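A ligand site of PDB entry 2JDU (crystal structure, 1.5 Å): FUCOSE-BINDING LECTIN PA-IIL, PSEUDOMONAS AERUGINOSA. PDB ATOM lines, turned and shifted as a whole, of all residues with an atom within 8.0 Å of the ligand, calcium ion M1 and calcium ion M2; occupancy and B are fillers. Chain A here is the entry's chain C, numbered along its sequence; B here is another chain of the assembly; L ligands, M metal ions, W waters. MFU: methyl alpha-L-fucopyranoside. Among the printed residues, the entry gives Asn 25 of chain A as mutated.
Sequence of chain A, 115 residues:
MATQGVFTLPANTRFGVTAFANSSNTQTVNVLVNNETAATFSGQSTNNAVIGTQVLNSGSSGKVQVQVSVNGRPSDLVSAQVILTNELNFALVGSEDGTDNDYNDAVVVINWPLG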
ATOM      1  N   ALA A  21       3.081 -21.739  19.232  1.00  0.00           N
ATOM      2  CA  ALA A  21       2.999 -22.257  20.619  1.00  0.00           C
ATOM      3  C   ALA A  21       3.695 -23.580  20.800  1.00  0.00           C
ATOM      4  O   ALA A  21       3.602 -24.445  19.945  1.00  0.00           O
ATOM      5  CB  ALA A  21       1.495 -22.415  21.049  1.00  0.00           C
ATOM      6  N   ASN A  22       4.380 -23.713  21.935  1.00  0.00           N
ATOM      7  CA  ASN A  22       5.062 -24.962  22.295  1.00  0.00           C
ATOM      8  C   ASN A  22       4.992 -25.149  23.809  1.00  0.00           C
ATOM      9  O   ASN A  22       6.003 -24.969  24.512  1.00  0.00           O
ATOM     10  CB  ASN A  22       6.528 -24.981  21.869  1.00  0.00           C
ATOM     11  CG  ASN A  22       6.666 -25.082  20.370  1.00  0.00           C
ATOM     12  OD1 ASN A  22       6.536 -26.154  19.801  1.00  0.00           O
ATOM     13  ND2 ASN A  22       6.944 -23.931  19.731  1.00  0.00           N
ATOM     14  N   SER A  23       3.787 -25.422  24.331  1.00  0.00           N
ATOM     15  CA  SER A  23       3.617 -25.498  25.798  1.00  0.00           C
ATOM     16  C   SER A  23       2.331 -26.255  26.089  1.00  0.00           C
ATOM     17  O   SER A  23       1.381 -26.219  25.302  1.00  0.00           O
ATOM     18  CB  SER A  23       3.540 -24.101  26.415  1.00  0.00           C
ATOM     19  OG  SER A  23       3.224 -24.204  27.815  1.00  0.00           O
ATOM     20  N   SER A  24       2.302 -26.967  27.216  1.00  0.00           N
ATOM     21  CA  SER A  24       1.057 -27.569  27.668  1.00  0.00           C
ATOM     22  C   SER A  24       0.057 -26.512  28.156  1.00  0.00           C
ATOM     23  O   SER A  24      -1.144 -26.831  28.268  1.00  0.00           O
ATOM     24  CB  SER A  24       1.303 -28.613  28.769  1.00  0.00           C
ATOM     25  OG  SER A  24       1.880 -28.047  29.912  1.00  0.00           O
ATOM     26  N   ASN A  25       0.503 -25.273  28.390  1.00  0.00           N
ATOM     27  CA  ASN A  25      -0.400 -24.227  28.830  1.00  0.00           C
ATOM     28  C   ASN A  25      -0.890 -23.377  27.655  1.00  0.00           C
ATOM     29  O   ASN A  25      -0.130 -23.135  26.689  1.00  0.00           O
ATOM     30  CB  ASN A  25       0.336 -23.258  29.751  1.00  0.00           C
ATOM     31  CG  ASN A  25       0.862 -23.906  30.995  1.00  0.00           C
ATOM     32  OD1 ASN A  25       0.089 -24.501  31.737  1.00  0.00           O
ATOM     33  ND2 ASN A  25       2.164 -23.736  31.280  1.00  0.00           N
ATOM     34  N   GLN A  27      -1.319 -20.166  25.617  1.00  0.00           N
ATOM     35  CA  GLN A  27      -0.543 -18.904  25.535  1.00  0.00           C
ATOM     36  C   GLN A  27      -1.475 -17.813  25.066  1.00  0.00           C
ATOM     37  O   GLN A  27      -2.380 -18.076  24.223  1.00  0.00           O
ATOM     38  CB  GLN A  27       0.553 -19.022  24.486  1.00  0.00           C
ATOM     39  CG  GLN A  27       1.456 -20.251  24.740  1.00  0.00           C
ATOM     40  CD  GLN A  27       2.241 -20.086  26.018  1.00  0.00           C
ATOM     41  OE1 GLN A  27       2.957 -19.094  26.157  1.00  0.00           O
ATOM     42  NE2 GLN A  27       2.195 -21.081  26.926  1.00  0.00           N
ATOM     43  N   GLN A  44      -3.096 -23.436  22.236  1.00  0.00           N
ATOM     44  CA  GLN A  44      -2.401 -24.387  23.086  1.00  0.00           C
ATOM     45  C   GLN A  44      -1.887 -25.548  22.221  1.00  0.00           C
ATOM     46  O   GLN A  44      -2.648 -26.389  21.729  1.00  0.00           O
ATOM     47  CB  GLN A  44      -3.288 -24.907  24.217  1.00  0.00           C
ATOM     48  CG  GLN A  44      -2.489 -25.688  25.290  1.00  0.00           C
ATOM     49  CD  GLN A  44      -2.333 -27.145  24.948  1.00  0.00           C
ATOM     50  OE1 GLN A  44      -3.336 -27.872  24.907  1.00  0.00           O
ATOM     51  NE2 GLN A  44      -1.084 -27.621  24.720  1.00  0.00           N
ATOM     52  N   SER A  45      -0.585 -25.572  22.000  1.00  0.00           N
ATOM     53  CA  SER A  45       0.043 -26.635  21.287  1.00  0.00           C
ATOM     54  C   SER A  45       1.436 -26.936  21.774  1.00  0.00           C
ATOM     55  O   SER A  45       2.113 -26.026  22.236  1.00  0.00           O
ATOM     56  CB  SER A  45       0.105 -26.231  19.781  1.00  0.00           C
ATOM     57  OG  SER A  45       0.961 -27.058  19.015  1.00  0.00           O
ATOM     58  N   THR A  46       1.841 -28.208  21.666  1.00  0.00           N
ATOM     59  CA  THR A  46       3.231 -28.554  21.924  1.00  0.00           C
ATOM     60  C   THR A  46       3.971 -28.940  20.637  1.00  0.00           C
ATOM     61  O   THR A  46       5.024 -29.571  20.690  1.00  0.00           O
ATOM     62  CB  THR A  46       3.361 -29.687  23.010  1.00  0.00           C
ATOM     63  OG1 THR A  46       2.521 -30.798  22.636  1.00  0.00           O
ATOM     64  CG2 THR A  46       2.953 -29.192  24.389  1.00  0.00           C
ATOM     65  N   ASN A  47       3.412 -28.553  19.466  1.00  0.00           N
ATOM     66  CA  ASN A  47       4.001 -28.914  18.180  1.00  0.00           C
ATOM     67  C   ASN A  47       3.990 -27.692  17.241  1.00  0.00           C
ATOM     68  O   ASN A  47       3.765 -27.819  16.029  1.00  0.00           O
ATOM     69  CB  ASN A  47       3.202 -30.072  17.563  1.00  0.00           C
ATOM     70  CG  ASN A  47       3.949 -30.801  16.470  1.00  0.00           C
ATOM     71  OD1 ASN A  47       5.161 -31.105  16.580  1.00  0.00           O
ATOM     72  ND2 ASN A  47       3.231 -31.096  15.396  1.00  0.00           N
ATOM     73  N   VAL A  70       0.262 -16.291  30.447  1.00  0.00           N
ATOM     74  CA  VAL A  70      -0.371 -17.603  30.599  1.00  0.00           C
ATOM     75  C   VAL A  70      -1.315 -17.434  31.775  1.00  0.00           C
ATOM     76  O   VAL A  70      -0.855 -17.155  32.896  1.00  0.00           O
ATOM     77  CB  VAL A  70       0.708 -18.688  30.799  1.00  0.00           C
ATOM     78  CG1 VAL A  70       0.089 -20.010  31.193  1.00  0.00           C
ATOM     79  CG2 VAL A  70       1.534 -18.797  29.515  1.00  0.00           C
ATOM     80  N   ARG A  73      -0.742 -14.421  33.977  1.00  0.00           N
ATOM     81  CA  ARG A  73       0.615 -14.315  34.495  1.00  0.00           C
ATOM     82  C   ARG A  73       1.606 -13.981  33.356  1.00  0.00           C
ATOM     83  O   ARG A  73       1.733 -14.769  32.419  1.00  0.00           O
ATOM     84  CB  ARG A  73       0.972 -15.655  35.164  1.00  0.00           C
ATOM     85  CG  ARG A  73      -0.118 -16.181  36.150  1.00  0.00           C
ATOM     86  CD  ARG A  73       0.289 -17.465  36.908  1.00  0.00           C
ATOM     87  NE  ARG A  73       0.101 -18.666  36.079  1.00  0.00           N
ATOM     88  CZ  ARG A  73       1.086 -19.387  35.551  1.00  0.00           C
ATOM     89  NH1 ARG A  73       2.354 -19.059  35.771  1.00  0.00           N
ATOM     90  NH2 ARG A  73       0.809 -20.450  34.806  1.00  0.00           N
ATOM     91  N   SER A  95       9.596 -16.817  24.901  1.00  0.00           N
ATOM     92  CA  SER A  95       8.940 -16.589  26.203  1.00  0.00           C
ATOM     93  C   SER A  95       8.928 -17.894  26.993  1.00  0.00           C
ATOM     94  O   SER A  95       8.931 -18.980  26.400  1.00  0.00           O
ATOM     95  CB  SER A  95       7.520 -16.056  26.062  1.00  0.00           C
ATOM     96  OG  SER A  95       6.697 -17.019  25.422  1.00  0.00           O
ATOM     97  N   GLU A  96       9.009 -17.758  28.326  1.00  0.00           N
ATOM     98  CA  GLU A  96       9.072 -18.899  29.224  1.00  0.00           C
ATOM     99  C   GLU A  96       7.983 -18.719  30.260  1.00  0.00           C
ATOM    100  O   GLU A  96       7.920 -17.709  30.936  1.00  0.00           O
ATOM    101  CB  GLU A  96      10.468 -18.939  29.921  1.00  0.00           C
ATOM    102  CG  GLU A  96      10.616 -20.138  30.927  1.00  0.00           C
ATOM    103  CD  GLU A  96      10.271 -21.478  30.281  1.00  0.00           C
ATOM    104  OE1 GLU A  96      10.835 -21.813  29.184  1.00  0.00           O
ATOM    105  OE2 GLU A  96       9.430 -22.241  30.850  1.00  0.00           O
ATOM    106  N   ASP A  97       7.130 -19.742  30.396  1.00  0.00           N
ATOM    107  CA  ASP A  97       5.977 -19.698  31.325  1.00  0.00           C
ATOM    108  C   ASP A  97       6.211 -20.636  32.503  1.00  0.00           C
ATOM    109  O   ASP A  97       5.308 -20.818  33.332  1.00  0.00           O
ATOM    110  CB  ASP A  97       4.663 -20.049  30.580  1.00  0.00           C
ATOM    111  CG  ASP A  97       4.609 -21.521  30.103  1.00  0.00           C
ATOM    112  OD1 ASP A  97       5.423 -22.397  30.530  1.00  0.00           O
ATOM    113  OD2 ASP A  97       3.717 -21.871  29.266  1.00  0.00           O
ATOM    114  N   GLY A  98       7.379 -21.254  32.576  1.00  0.00           N
ATOM    115  CA  GLY A  98       7.518 -22.465  33.411  1.00  0.00           C
ATOM    116  C   GLY A  98       8.898 -22.602  33.984  1.00  0.00           C
ATOM    117  O   GLY A  98       9.548 -21.598  34.294  1.00  0.00           O
ATOM    118  N   THR A  99       9.355 -23.852  34.089  1.00  0.00           N
ATOM    119  CA  THR A  99      10.576 -24.149  34.857  1.00  0.00           C
ATOM    120  C   THR A  99      11.699 -24.738  34.017  1.00  0.00           C
ATOM    121  O   THR A  99      12.831 -24.862  34.506  1.00  0.00           O
ATOM    122  CB  THR A  99      10.287 -25.079  36.105  1.00  0.00           C
ATOM    123  OG1 THR A  99       9.732 -26.331  35.671  1.00  0.00           O
ATOM    124  CG2 THR A  99       9.303 -24.431  37.093  1.00  0.00           C
ATOM    125  N   ASP A 100      11.421 -25.100  32.757  1.00  0.00           N
ATOM    126  CA  ASP A 100      12.414 -25.863  31.998  1.00  0.00           C
ATOM    127  C   ASP A 100      13.333 -25.003  31.139  1.00  0.00           C
ATOM    128  O   ASP A 100      14.306 -25.507  30.561  1.00  0.00           O
ATOM    129  CB  ASP A 100      11.777 -26.962  31.151  1.00  0.00           C
ATOM    130  CG  ASP A 100      10.901 -26.408  30.043  1.00  0.00           C
ATOM    131  OD1 ASP A 100      10.557 -25.200  30.071  1.00  0.00           O
ATOM    132  OD2 ASP A 100      10.555 -27.211  29.158  1.00  0.00           O
ATOM    133  N   ASN A 101      13.009 -23.705  31.045  1.00  0.00           N
ATOM    134  CA  ASN A 101      13.815 -22.723  30.302  1.00  0.00           C
ATOM    135  C   ASN A 101      14.148 -23.043  28.831  1.00  0.00           C
ATOM    136  O   ASN A 101      15.260 -22.790  28.386  1.00  0.00           O
ATOM    137  CB  ASN A 101      15.090 -22.402  31.089  1.00  0.00           C
ATOM    138  CG  ASN A 101      14.763 -21.918  32.486  1.00  0.00           C
ATOM    139  OD1 ASN A 101      13.824 -21.136  32.689  1.00  0.00           O
ATOM    140  ND2 ASN A 101      15.525 -22.401  33.455  1.00  0.00           N
ATOM    141  N   ASP A 102      13.163 -23.573  28.121  1.00  0.00           N
ATOM    142  CA  ASP A 102      13.308 -23.706  26.673  1.00  0.00           C
ATOM    143  C   ASP A 102      13.013 -22.373  25.933  1.00  0.00           C
ATOM    144  O   ASP A 102      13.423 -22.237  24.787  1.00  0.00           O
ATOM    145  CB  ASP A 102      12.573 -24.937  26.102  1.00  0.00           C
ATOM    146  CG  ASP A 102      11.065 -24.997  26.422  1.00  0.00           C
ATOM    147  OD1 ASP A 102      10.520 -24.104  27.094  1.00  0.00           O
ATOM    148  OD2 ASP A 102      10.425 -25.982  25.941  1.00  0.00           O
ATOM    149  N   TYR A 103      12.352 -21.403  26.602  1.00  0.00           N
ATOM    150  CA  TYR A 103      11.937 -20.094  26.004  1.00  0.00           C
ATOM    151  C   TYR A 103      11.207 -20.221  24.660  1.00  0.00           C
ATOM    152  O   TYR A 103      11.150 -19.237  23.884  1.00  0.00           O
ATOM    153  CB  TYR A 103      13.110 -19.053  25.924  1.00  0.00           C
ATOM    154  CG  TYR A 103      13.324 -18.444  27.287  1.00  0.00           C
ATOM    155  CD1 TYR A 103      12.758 -17.207  27.627  1.00  0.00           C
ATOM    156  CD2 TYR A 103      14.035 -19.155  28.271  1.00  0.00           C
ATOM    157  CE1 TYR A 103      12.889 -16.675  28.935  1.00  0.00           C
ATOM    158  CE2 TYR A 103      14.184 -18.622  29.550  1.00  0.00           C
ATOM    159  CZ  TYR A 103      13.641 -17.421  29.862  1.00  0.00           C
ATOM    160  OH  TYR A 103      13.829 -17.037  31.175  1.00  0.00           O
ATOM    161  N   ASN A 104      10.489 -21.351  24.501  1.00  0.00           N
ATOM    162  CA  ASN A 104       9.772 -21.576  23.252  1.00  0.00           C
ATOM    163  C   ASN A 104       8.276 -21.653  23.511  1.00  0.00           C
ATOM    164  O   ASN A 104       7.535 -22.023  22.591  1.00  0.00           O
ATOM    165  CB  ASN A 104      10.255 -22.844  22.549  1.00  0.00           C
ATOM    166  CG  ASN A 104       9.814 -24.110  23.278  1.00  0.00           C
ATOM    167  OD1 ASN A 104       9.250 -24.018  24.401  1.00  0.00           O
ATOM    168  ND2 ASN A 104      10.036 -25.267  22.672  1.00  0.00           N
ATOM    169  N   ASP A 105       7.831 -21.241  24.699  1.00  0.00           N
ATOM    170  CA  ASP A 105       6.443 -21.575  25.074  1.00  0.00           C
ATOM    171  C   ASP A 105       5.478 -20.800  24.169  1.00  0.00           C
ATOM    172  O   ASP A 105       4.479 -21.350  23.703  1.00  0.00           O
ATOM    173  CB  ASP A 105       6.197 -21.311  26.558  1.00  0.00           C
ATOM    174  CG  ASP A 105       7.034 -22.207  27.432  1.00  0.00           C
ATOM    175  OD1 ASP A 105       7.250 -23.363  27.008  1.00  0.00           O
ATOM    176  OD2 ASP A 105       7.466 -21.726  28.499  1.00  0.00           O
ATOM    177  N   ALA A 106       5.798 -19.536  23.918  1.00  0.00           N
ATOM    178  CA  ALA A 106       5.284 -18.820  22.745  1.00  0.00           C
ATOM    179  C   ALA A 106       6.477 -18.154  22.083  1.00  0.00           C
ATOM    180  O   ALA A 106       7.309 -17.518  22.746  1.00  0.00           O
ATOM    181  CB  ALA A 106       4.229 -17.759  23.109  1.00  0.00           C
ATOM    182  N   PRO B 113      14.147 -25.399  19.817  1.00  0.00           N
ATOM    183  CA  PRO B 113      13.409 -26.667  19.943  1.00  0.00           C
ATOM    184  C   PRO B 113      11.915 -26.437  19.972  1.00  0.00           C
ATOM    185  O   PRO B 113      11.414 -25.307  20.206  1.00  0.00           O
ATOM    186  CB  PRO B 113      13.808 -27.177  21.330  1.00  0.00           C
ATOM    187  CG  PRO B 113      14.056 -25.938  22.151  1.00  0.00           C
ATOM    188  CD  PRO B 113      14.642 -24.890  21.131  1.00  0.00           C
ATOM    189  N   LEU B 114      11.186 -27.521  19.760  1.00  0.00           N
ATOM    190  CA  LEU B 114       9.719 -27.512  19.868  1.00  0.00           C
ATOM    191  C   LEU B 114       9.330 -28.227  21.176  1.00  0.00           C
ATOM    192  O   LEU B 114      10.177 -28.767  21.882  1.00  0.00           O
ATOM    193  CB  LEU B 114       9.061 -28.263  18.703  1.00  0.00           C
ATOM    194  CG  LEU B 114       9.470 -27.725  17.334  1.00  0.00           C
ATOM    195  CD1 LEU B 114       8.614 -28.468  16.282  1.00  0.00           C
ATOM    196  CD2 LEU B 114       9.316 -26.232  17.218  1.00  0.00           C
ATOM    197  N   GLY B 115       8.025 -28.232  21.477  1.00  0.00           N
ATOM    198  CA  GLY B 115       7.547 -29.068  22.586  1.00  0.00           C
ATOM    199  C   GLY B 115       7.469 -28.351  23.910  1.00  0.00           C
ATOM    200  O   GLY B 115       8.136 -27.313  24.067  1.00  0.00           O
ATOM    201  OXT GLY B 115       6.754 -28.835  24.829  1.00  0.00           O
HETATM  202  C1  MFU L   1       5.206 -26.050  29.774  1.00  0.00           C
HETATM  203  C2  MFU L   1       6.433 -25.466  29.137  1.00  0.00           C
HETATM  204  C3  MFU L   1       7.431 -26.602  28.783  1.00  0.00           C
HETATM  205  C4  MFU L   1       6.821 -27.737  27.967  1.00  0.00           C
HETATM  206  C5  MFU L   1       5.604 -28.235  28.721  1.00  0.00           C
HETATM  207  C6  MFU L   1       4.948 -29.469  28.064  1.00  0.00           C
HETATM  208  O1  MFU L   1       5.560 -26.576  31.070  1.00  0.00           O
HETATM  209  O2  MFU L   1       7.102 -24.483  29.967  1.00  0.00           O
HETATM  210  O3  MFU L   1       8.486 -25.994  28.011  1.00  0.00           O
HETATM  211  O4  MFU L   1       6.512 -27.221  26.651  1.00  0.00           O
HETATM  212  O5  MFU L   1       4.691 -27.128  28.937  1.00  0.00           O
HETATM  213  CM  MFU L   1       4.339 -26.841  31.829  1.00  0.00           C
HETATM  214 CA    CA M   1       9.090 -23.743  28.878  1.00  0.00          CA
HETATM  215 CA    CA M   2       8.031 -25.469  25.764  1.00  0.00          CA
HETATM  216  O   HOH W   1       8.117 -25.880  32.458  1.00  0.00           O
HETATM  217  O   HOH W   2       3.229 -30.073  31.183  1.00  0.00           O
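OG of Ser 24 is in hydrogen-bond range of O5 of the ligand (3.1 Å). OG of Ser 23 lies close to O5 of the ligand. O2 of the ligand lies close to OD1 of Asp 97 (2.7 Å). The backbone NH (N) of Ser 24 lies within hydrogen-bond range of an oxygen (O5) of the ligand (2.9 Å).
The side-chain hydroxyl of Ser 23 sits at hydrogen-bond distance from the backbone NH of Asn 25 (3.0 Å). The backbone NH of Tyr 103 lies close to the side-chain carboxylate of Glu 96, at 3.0 Å. The backbone carbonyl oxygen (O) of Thr 46 sits close to the backbone NH (N) of Gly 115 of chain B, at 3.4 Å. The backbone NH (N) of Ser 23 is in hydrogen-bond range of the backbone carbonyl oxygen (O) of Ser 45. The side-chain carboxylate of Asp 105 sits close to the backbone NH of Asp 97 (2.8 Å). The side-chain carboxylate (OE2) of Glu 96 lies close to the backbone NH (N) of Gly 98. The side-chain hydroxyl of Ser 23 sits close to the side-chain amide nitrogen of Gln 27 (3.4 Å). N of Asn 22 lies close to O of Ser 45, 3.3 Å away.
Asn 25 touches the ligand (ND2 to CM, 3.8 Å). Of the 27 residues printed, 10 come within 4 Å of the ligand.
Four residues have an atom within 4 Å of calcium ion M1: Glu 96, Asp 100, Asp 102 and Asp 105.
Within 4 Å of calcium ion M2: Asn 22, Asp 102, Asn 104, Asp 105 and Gly 115 of chain B.
Calcium ion M1 is bound by OD1 of Asp 102, O2 of the ligand, OD1 of Asp 100, O3 of the ligand, OE2 of Glu 96, OD2 of Asp 105, OE1 of Glu 96 and OD1 of Asp 105.
Calcium ion M2 is bound by the side-chain amide oxygen (OD1) of Asn 104 (2.3 Å), an oxygen (O3) of the ligand (2.4 Å), the backbone carbonyl oxygen (O) of Asn 22 (2.4 Å), the side-chain carboxylate (OD2) of Asp 102 (2.5 Å), an oxygen (O4) of the ligand (2.5 Å), the chain-end carboxylate (O) of Gly 115 of chain B (2.5 Å) and the side-chain carboxylate (OD1) of Asp 105 (2.6 Å). Calcium ion M2 has seven donor atoms within binding distance. Slightly farther from calcium ion M2 lies the side-chain carboxylate (OD1) of Asp 102 (3.1 Å).
Water W1 lies within hydrogen-bond range of the backbone NH of Thr 99 (2.9 Å), an oxygen (O1) of the ligand (3.0 Å) and the backbone NH of Asp 100 (3.4 Å).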
